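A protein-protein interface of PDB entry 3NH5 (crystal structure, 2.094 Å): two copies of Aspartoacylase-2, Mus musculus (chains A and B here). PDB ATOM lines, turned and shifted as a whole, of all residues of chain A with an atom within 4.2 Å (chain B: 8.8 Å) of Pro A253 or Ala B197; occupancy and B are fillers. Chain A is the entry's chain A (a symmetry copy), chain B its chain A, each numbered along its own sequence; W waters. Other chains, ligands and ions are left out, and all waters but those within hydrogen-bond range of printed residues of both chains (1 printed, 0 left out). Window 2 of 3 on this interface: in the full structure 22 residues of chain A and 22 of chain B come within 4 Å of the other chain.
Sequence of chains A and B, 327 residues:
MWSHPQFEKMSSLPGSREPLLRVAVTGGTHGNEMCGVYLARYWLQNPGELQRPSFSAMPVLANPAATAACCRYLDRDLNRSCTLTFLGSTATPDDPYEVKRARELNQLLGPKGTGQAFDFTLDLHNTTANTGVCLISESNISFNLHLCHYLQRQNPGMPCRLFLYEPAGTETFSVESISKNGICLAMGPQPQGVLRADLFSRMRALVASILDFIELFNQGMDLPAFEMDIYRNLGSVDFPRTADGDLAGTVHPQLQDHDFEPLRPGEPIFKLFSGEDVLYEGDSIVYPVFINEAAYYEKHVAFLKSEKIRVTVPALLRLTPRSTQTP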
ATOM      1  N   THR A 250      14.078  11.804   9.898  1.00  0.00           N
ATOM      2  CA  THR A 250      14.140  11.573   8.462  1.00  0.00           C
ATOM      3  C   THR A 250      13.755  12.829   7.686  1.00  0.00           C
ATOM      4  O   THR A 250      13.482  13.888   8.271  1.00  0.00           O
ATOM      5  CB  THR A 250      13.289  10.359   8.010  1.00  0.00           C
ATOM      6  OG1 THR A 250      13.604  10.025   6.648  1.00  0.00           O
ATOM      7  CG2 THR A 250      11.796  10.651   8.155  1.00  0.00           C
ATOM      8  N   VAL A 251      13.765  12.705   6.364  1.00  0.00           N
ATOM      9  CA  VAL A 251      13.487  13.823   5.483  1.00  0.00           C
ATOM     10  C   VAL A 251      12.115  14.409   5.806  1.00  0.00           C
ATOM     11  O   VAL A 251      11.122  13.683   5.924  1.00  0.00           O
ATOM     12  CB  VAL A 251      13.568  13.378   3.986  1.00  0.00           C
ATOM     13  CG1 VAL A 251      13.137  14.503   3.053  1.00  0.00           C
ATOM     14  CG2 VAL A 251      14.990  12.896   3.654  1.00  0.00           C
ATOM     15  N   HIS A 252      12.073  15.728   5.931  1.00  0.00           N
ATOM     16  CA  HIS A 252      10.859  16.448   6.292  1.00  0.00           C
ATOM     17  C   HIS A 252       9.785  16.251   5.243  1.00  0.00           C
ATOM     18  O   HIS A 252      10.092  16.161   4.052  1.00  0.00           O
ATOM     19  CB  HIS A 252      11.178  17.938   6.474  1.00  0.00           C
ATOM     20  CG  HIS A 252      10.139  18.695   7.237  1.00  0.00           C
ATOM     21  ND1 HIS A 252       8.945  19.098   6.674  1.00  0.00           N
ATOM     22  CD2 HIS A 252      10.110  19.117   8.528  1.00  0.00           C
ATOM     23  CE1 HIS A 252       8.225  19.734   7.584  1.00  0.00           C
ATOM     24  NE2 HIS A 252       8.910  19.760   8.716  1.00  0.00           N
ATOM     25  N   PRO A 253       8.513  16.169   5.672  1.00  0.00           N
ATOM     26  CA  PRO A 253       7.431  15.957   4.704  1.00  0.00           C
ATOM     27  C   PRO A 253       7.350  17.035   3.623  1.00  0.00           C
ATOM     28  O   PRO A 253       6.843  16.761   2.534  1.00  0.00           O
ATOM     29  CB  PRO A 253       6.167  15.979   5.575  1.00  0.00           C
ATOM     30  CG  PRO A 253       6.641  15.525   6.931  1.00  0.00           C
ATOM     31  CD  PRO A 253       8.032  16.115   7.068  1.00  0.00           C
ATOM     32  N   GLN A 254       7.842  18.236   3.908  1.00  0.00           N
ATOM     33  CA  GLN A 254       7.748  19.323   2.942  1.00  0.00           C
ATOM     34  C   GLN A 254       8.884  19.288   1.921  1.00  0.00           C
ATOM     35  O   GLN A 254       8.833  19.965   0.892  1.00  0.00           O
ATOM     36  CB  GLN A 254       7.698  20.677   3.649  1.00  0.00           C
ATOM     37  CG  GLN A 254       6.337  20.980   4.254  1.00  0.00           C
ATOM     38  CD  GLN A 254       6.295  22.326   4.951  1.00  0.00           C
ATOM     39  OE1 GLN A 254       7.142  23.192   4.712  1.00  0.00           O
ATOM     40  NE2 GLN A 254       5.303  22.509   5.823  1.00  0.00           N
ATOM     41  N   LEU A 255       9.908  18.505   2.223  1.00  0.00           N
ATOM     42  CA  LEU A 255      11.020  18.318   1.317  1.00  0.00           C
ATOM     43  C   LEU A 255      10.817  17.020   0.537  1.00  0.00           C
ATOM     44  O   LEU A 255      11.116  16.941  -0.654  1.00  0.00           O
ATOM     45  CB  LEU A 255      12.325  18.281   2.098  1.00  0.00           C
ATOM     46  CG  LEU A 255      13.583  17.992   1.293  1.00  0.00           C
ATOM     47  CD1 LEU A 255      13.797  19.066   0.210  1.00  0.00           C
ATOM     48  CD2 LEU A 255      14.765  17.926   2.233  1.00  0.00           C
ATOM     49  N   GLN A 256      10.280  16.012   1.220  1.00  0.00           N
ATOM     50  CA  GLN A 256      10.056  14.705   0.635  1.00  0.00           C
ATOM     51  C   GLN A 256       9.367  14.817  -0.728  1.00  0.00           C
ATOM     52  O   GLN A 256       8.342  15.486  -0.852  1.00  0.00           O
ATOM     53  CB  GLN A 256       9.227  13.825   1.588  1.00  0.00           C
ATOM     54  CG  GLN A 256       8.875  12.444   1.040  1.00  0.00           C
ATOM     55  CD  GLN A 256      10.086  11.549   0.884  1.00  0.00           C
ATOM     56  OE1 GLN A 256      10.827  11.314   1.847  1.00  0.00           O
ATOM     57  NE2 GLN A 256      10.313  11.056  -0.344  1.00  0.00           N
ATOM     58  N   CYS B  35       9.215   1.816   9.152  1.00  0.00           N
ATOM     59  CA  CYS B  35       8.450   2.491  10.206  1.00  0.00           C
ATOM     60  C   CYS B  35       8.571   1.686  11.495  1.00  0.00           C
ATOM     61  O   CYS B  35       8.928   2.228  12.543  1.00  0.00           O
ATOM     62  CB  CYS B  35       6.975   2.677   9.830  1.00  0.00           C
ATOM     63  SG  CYS B  35       6.694   3.870   8.485  1.00  0.00           S
ATOM     64  N   MET B 187       1.216  -0.512   6.532  1.00  0.00           N
ATOM     65  CA  MET B 187       1.076   0.781   5.871  1.00  0.00           C
ATOM     66  C   MET B 187       1.933   0.919   4.608  1.00  0.00           C
ATOM     67  O   MET B 187       3.131   0.609   4.603  1.00  0.00           O
ATOM     68  CB  MET B 187       1.337   1.932   6.843  1.00  0.00           C
ATOM     69  CG  MET B 187       0.263   1.995   7.929  1.00  0.00           C
ATOM     70  SD  MET B 187       0.589   3.251   9.152  1.00  0.00           S
ATOM     71  CE  MET B 187       0.513   4.752   8.167  1.00  0.00           C
ATOM     72  N   GLN B 190       5.459   2.369   0.713  1.00  0.00           N
ATOM     73  CA  GLN B 190       6.767   2.838   1.149  1.00  0.00           C
ATOM     74  C   GLN B 190       7.838   1.892   0.623  1.00  0.00           C
ATOM     75  O   GLN B 190       7.744   0.682   0.801  1.00  0.00           O
ATOM     76  CB  GLN B 190       6.854   2.941   2.688  1.00  0.00           C
ATOM     77  CG  GLN B 190       8.130   3.603   3.174  1.00  0.00           C
ATOM     78  CD  GLN B 190       8.154   3.838   4.678  1.00  0.00           C
ATOM     79  OE1 GLN B 190       8.021   4.975   5.135  1.00  0.00           O
ATOM     80  NE2 GLN B 190       8.337   2.765   5.452  1.00  0.00           N
ATOM     81  N   VAL B 194      13.437   2.703   3.018  1.00  0.00           N
ATOM     82  CA  VAL B 194      13.193   4.148   3.082  1.00  0.00           C
ATOM     83  C   VAL B 194      12.247   4.426   4.235  1.00  0.00           C
ATOM     84  O   VAL B 194      11.252   3.721   4.403  1.00  0.00           O
ATOM     85  CB  VAL B 194      12.544   4.710   1.785  1.00  0.00           C
ATOM     86  CG1 VAL B 194      12.082   6.136   2.009  1.00  0.00           C
ATOM     87  CG2 VAL B 194      13.509   4.627   0.581  1.00  0.00           C
ATOM     88  N   LEU B 195      12.570   5.441   5.025  1.00  0.00           N
ATOM     89  CA  LEU B 195      11.684   5.938   6.064  1.00  0.00           C
ATOM     90  C   LEU B 195      11.084   7.270   5.642  1.00  0.00           C
ATOM     91  O   LEU B 195      11.787   8.283   5.554  1.00  0.00           O
ATOM     92  CB  LEU B 195      12.453   6.135   7.390  1.00  0.00           C
ATOM     93  CG  LEU B 195      11.603   6.589   8.583  1.00  0.00           C
ATOM     94  CD1 LEU B 195      10.520   5.545   8.872  1.00  0.00           C
ATOM     95  CD2 LEU B 195      12.440   6.820   9.832  1.00  0.00           C
ATOM     96  N   ARG B 196       9.787   7.276   5.391  1.00  0.00           N
ATOM     97  CA  ARG B 196       9.080   8.520   5.128  1.00  0.00           C
ATOM     98  C   ARG B 196       8.545   9.133   6.433  1.00  0.00           C
ATOM     99  O   ARG B 196       7.945   8.435   7.241  1.00  0.00           O
ATOM    100  CB  ARG B 196       7.915   8.261   4.171  1.00  0.00           C
ATOM    101  CG  ARG B 196       8.333   7.786   2.762  1.00  0.00           C
ATOM    102  CD  ARG B 196       7.109   7.549   1.882  1.00  0.00           C
ATOM    103  NE  ARG B 196       6.334   8.781   1.753  1.00  0.00           N
ATOM    104  CZ  ARG B 196       6.407   9.617   0.720  1.00  0.00           C
ATOM    105  NH1 ARG B 196       7.204   9.349  -0.317  1.00  0.00           N
ATOM    106  NH2 ARG B 196       5.667  10.719   0.717  1.00  0.00           N
ATOM    107  N   ALA B 197       8.766  10.431   6.632  1.00  0.00           N
ATOM    108  CA  ALA B 197       8.262  11.118   7.809  1.00  0.00           C
ATOM    109  C   ALA B 197       6.741  10.990   7.905  1.00  0.00           C
ATOM    110  O   ALA B 197       6.203  10.835   8.999  1.00  0.00           O
ATOM    111  CB  ALA B 197       8.691  12.591   7.812  1.00  0.00           C
ATOM    112  N   ASP B 198       6.044  11.033   6.770  1.00  0.00           N
ATOM    113  CA  ASP B 198       4.583  10.988   6.811  1.00  0.00           C
ATOM    114  C   ASP B 198       4.041   9.666   7.354  1.00  0.00           C
ATOM    115  O   ASP B 198       3.193   9.658   8.258  1.00  0.00           O
ATOM    116  CB  ASP B 198       3.897  11.425   5.489  1.00  0.00           C
ATOM    117  CG  ASP B 198       4.306  10.584   4.243  1.00  0.00           C
ATOM    118  OD1 ASP B 198       5.069   9.598   4.338  1.00  0.00           O
ATOM    119  OD2 ASP B 198       3.835  10.929   3.129  1.00  0.00           O
ATOM    120  N   LEU B 199       4.545   8.550   6.836  1.00  0.00           N
ATOM    121  CA  LEU B 199       4.121   7.250   7.348  1.00  0.00           C
ATOM    122  C   LEU B 199       4.624   6.957   8.763  1.00  0.00           C
ATOM    123  O   LEU B 199       3.948   6.288   9.536  1.00  0.00           O
ATOM    124  CB  LEU B 199       4.528   6.126   6.408  1.00  0.00           C
ATOM    125  CG  LEU B 199       3.866   6.177   5.026  1.00  0.00           C
ATOM    126  CD1 LEU B 199       4.525   5.171   4.081  1.00  0.00           C
ATOM    127  CD2 LEU B 199       2.365   5.927   5.121  1.00  0.00           C
ATOM    128  N   PHE B 200       5.810   7.443   9.100  1.00  0.00           N
ATOM    129  CA  PHE B 200       6.308   7.258  10.452  1.00  0.00           C
ATOM    130  C   PHE B 200       5.347   7.900  11.468  1.00  0.00           C
ATOM    131  O   PHE B 200       4.917   7.239  12.412  1.00  0.00           O
ATOM    132  CB  PHE B 200       7.704   7.849  10.581  1.00  0.00           C
ATOM    133  CG  PHE B 200       8.311   7.707  11.955  1.00  0.00           C
ATOM    134  CD1 PHE B 200       8.908   6.508  12.349  1.00  0.00           C
ATOM    135  CD2 PHE B 200       8.308   8.781  12.846  1.00  0.00           C
ATOM    136  CE1 PHE B 200       9.499   6.382  13.621  1.00  0.00           C
ATOM    137  CE2 PHE B 200       8.887   8.664  14.116  1.00  0.00           C
ATOM    138  CZ  PHE B 200       9.481   7.467  14.501  1.00  0.00           C
ATOM    139  N   SER B 201       4.998   9.174  11.258  1.00  0.00           N
ATOM    140  CA  SER B 201       4.096   9.886  12.155  1.00  0.00           C
ATOM    141  C   SER B 201       2.727   9.252  12.229  1.00  0.00           C
ATOM    142  O   SER B 201       2.167   9.120  13.319  1.00  0.00           O
ATOM    143  CB  SER B 201       3.921  11.346  11.734  1.00  0.00           C
ATOM    144  OG  SER B 201       5.130  12.041  11.904  1.00  0.00           O
ATOM    145  N   ARG B 202       2.177   8.886  11.073  1.00  0.00           N
ATOM    146  CA  ARG B 202       0.833   8.338  11.043  1.00  0.00           C
ATOM    147  C   ARG B 202       0.799   7.010  11.777  1.00  0.00           C
ATOM    148  O   ARG B 202      -0.112   6.757  12.556  1.00  0.00           O
ATOM    149  CB  ARG B 202       0.316   8.163   9.611  1.00  0.00           C
ATOM    150  CG  ARG B 202      -1.182   7.840   9.544  1.00  0.00           C
ATOM    151  CD  ARG B 202      -1.758   8.071   8.137  1.00  0.00           C
ATOM    152  NE  ARG B 202      -1.386   9.385   7.602  1.00  0.00           N
ATOM    153  CZ  ARG B 202      -0.724   9.582   6.460  1.00  0.00           C
ATOM    154  NH1 ARG B 202      -0.366   8.550   5.702  1.00  0.00           N
ATOM    155  NH2 ARG B 202      -0.429  10.817   6.065  1.00  0.00           N
ATOM    156  N   MET B 203       1.791   6.162  11.521  1.00  0.00           N
ATOM    157  CA  MET B 203       1.834   4.863  12.163  1.00  0.00           C
ATOM    158  C   MET B 203       1.971   5.048  13.678  1.00  0.00           C
ATOM    159  O   MET B 203       1.355   4.325  14.463  1.00  0.00           O
ATOM    160  CB  MET B 203       2.980   4.000  11.637  1.00  0.00           C
ATOM    161  CG  MET B 203       2.974   2.602  12.237  1.00  0.00           C
ATOM    162  SD  MET B 203       4.268   1.485  11.666  1.00  0.00           S
ATOM    163  CE  MET B 203       3.573   0.908  10.111  1.00  0.00           C
ATOM    164  N   ARG B 204       2.776   6.029  14.058  1.00  0.00           N
ATOM    165  CA  ARG B 204       3.024   6.340  15.444  1.00  0.00           C
ATOM    166  C   ARG B 204       1.733   6.761  16.159  1.00  0.00           C
ATOM    167  O   ARG B 204       1.492   6.364  17.304  1.00  0.00           O
ATOM    168  CB  ARG B 204       4.060   7.450  15.532  1.00  0.00           C
ATOM    169  CG  ARG B 204       4.413   7.872  16.946  1.00  0.00           C
ATOM    170  CD  ARG B 204       5.574   8.882  16.908  1.00  0.00           C
ATOM    171  NE  ARG B 204       6.083   9.172  18.245  1.00  0.00           N
ATOM    172  CZ  ARG B 204       7.102   9.988  18.508  1.00  0.00           C
ATOM    173  NH1 ARG B 204       7.740  10.615  17.528  1.00  0.00           N
ATOM    174  NH2 ARG B 204       7.489  10.175  19.761  1.00  0.00           N
HETATM  175  O   HOH W   1       9.974  11.996   4.461  1.00  0.00           O
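Thr A250 touches Arg B196 (CG2 to C, 3.98 Å). CG2 of Thr A250 touches N of Ala B197, 3.4 Å away. Ala B197 touches Val A251 (CB to O, 3.3 Å). Pro A253 touches Ala B197 (CD to CB, 3.7 Å). NH1 of Arg B196 touches NE2 of Gln A256, 3.5 Å away.
The side-chain hydroxyl of Thr A250 lies within hydrogen-bond range of the backbone carbonyl oxygen of Leu B195, at 2.7 Å.
Of the 7 printed residues of chain A, 4 touch a printed residue of chain B. Hydrophobic or aromatic side chains of chain A within 4 Å of the printed part of chain B: Pro A253.
N of Arg B196 is in hydrogen-bond range of OE1 of Gln B190, at 2.9 Å. O of Ala B197 is in hydrogen-bond range of OG of Ser B201. NE of Arg B196 lies within salt-bridge range of OD1 of Asp B198.
Water W1 lies within hydrogen-bond range of the backbone carbonyl oxygen of Val A251 (2.5 Å), the side-chain amide oxygen of Gln A256 (2.8 Å) and the backbone NH of Ala B197 (2.9 Å).
Pro A253 touches just one residue of chain B: Ala B197. Ala B197 touches just these residues of chain A: Thr A250, Val A251 and Pro A253. Of the printed residues of chain B, Gln A256 touches Arg B196 (3.5 Å). Printed residues of chain B within 4 Å of Val A251: Ala B197. Printed residues of chain A within 4 Å of Leu B195: Thr A250. Cys B35 touches none of the printed residues of chain A. Arg B204 touches none of the printed residues of chain A.
No position is printed for both chains. Of the 6 pairs that touch across the chains among the printed residues, none has its exchanged pair printed and touching as well.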
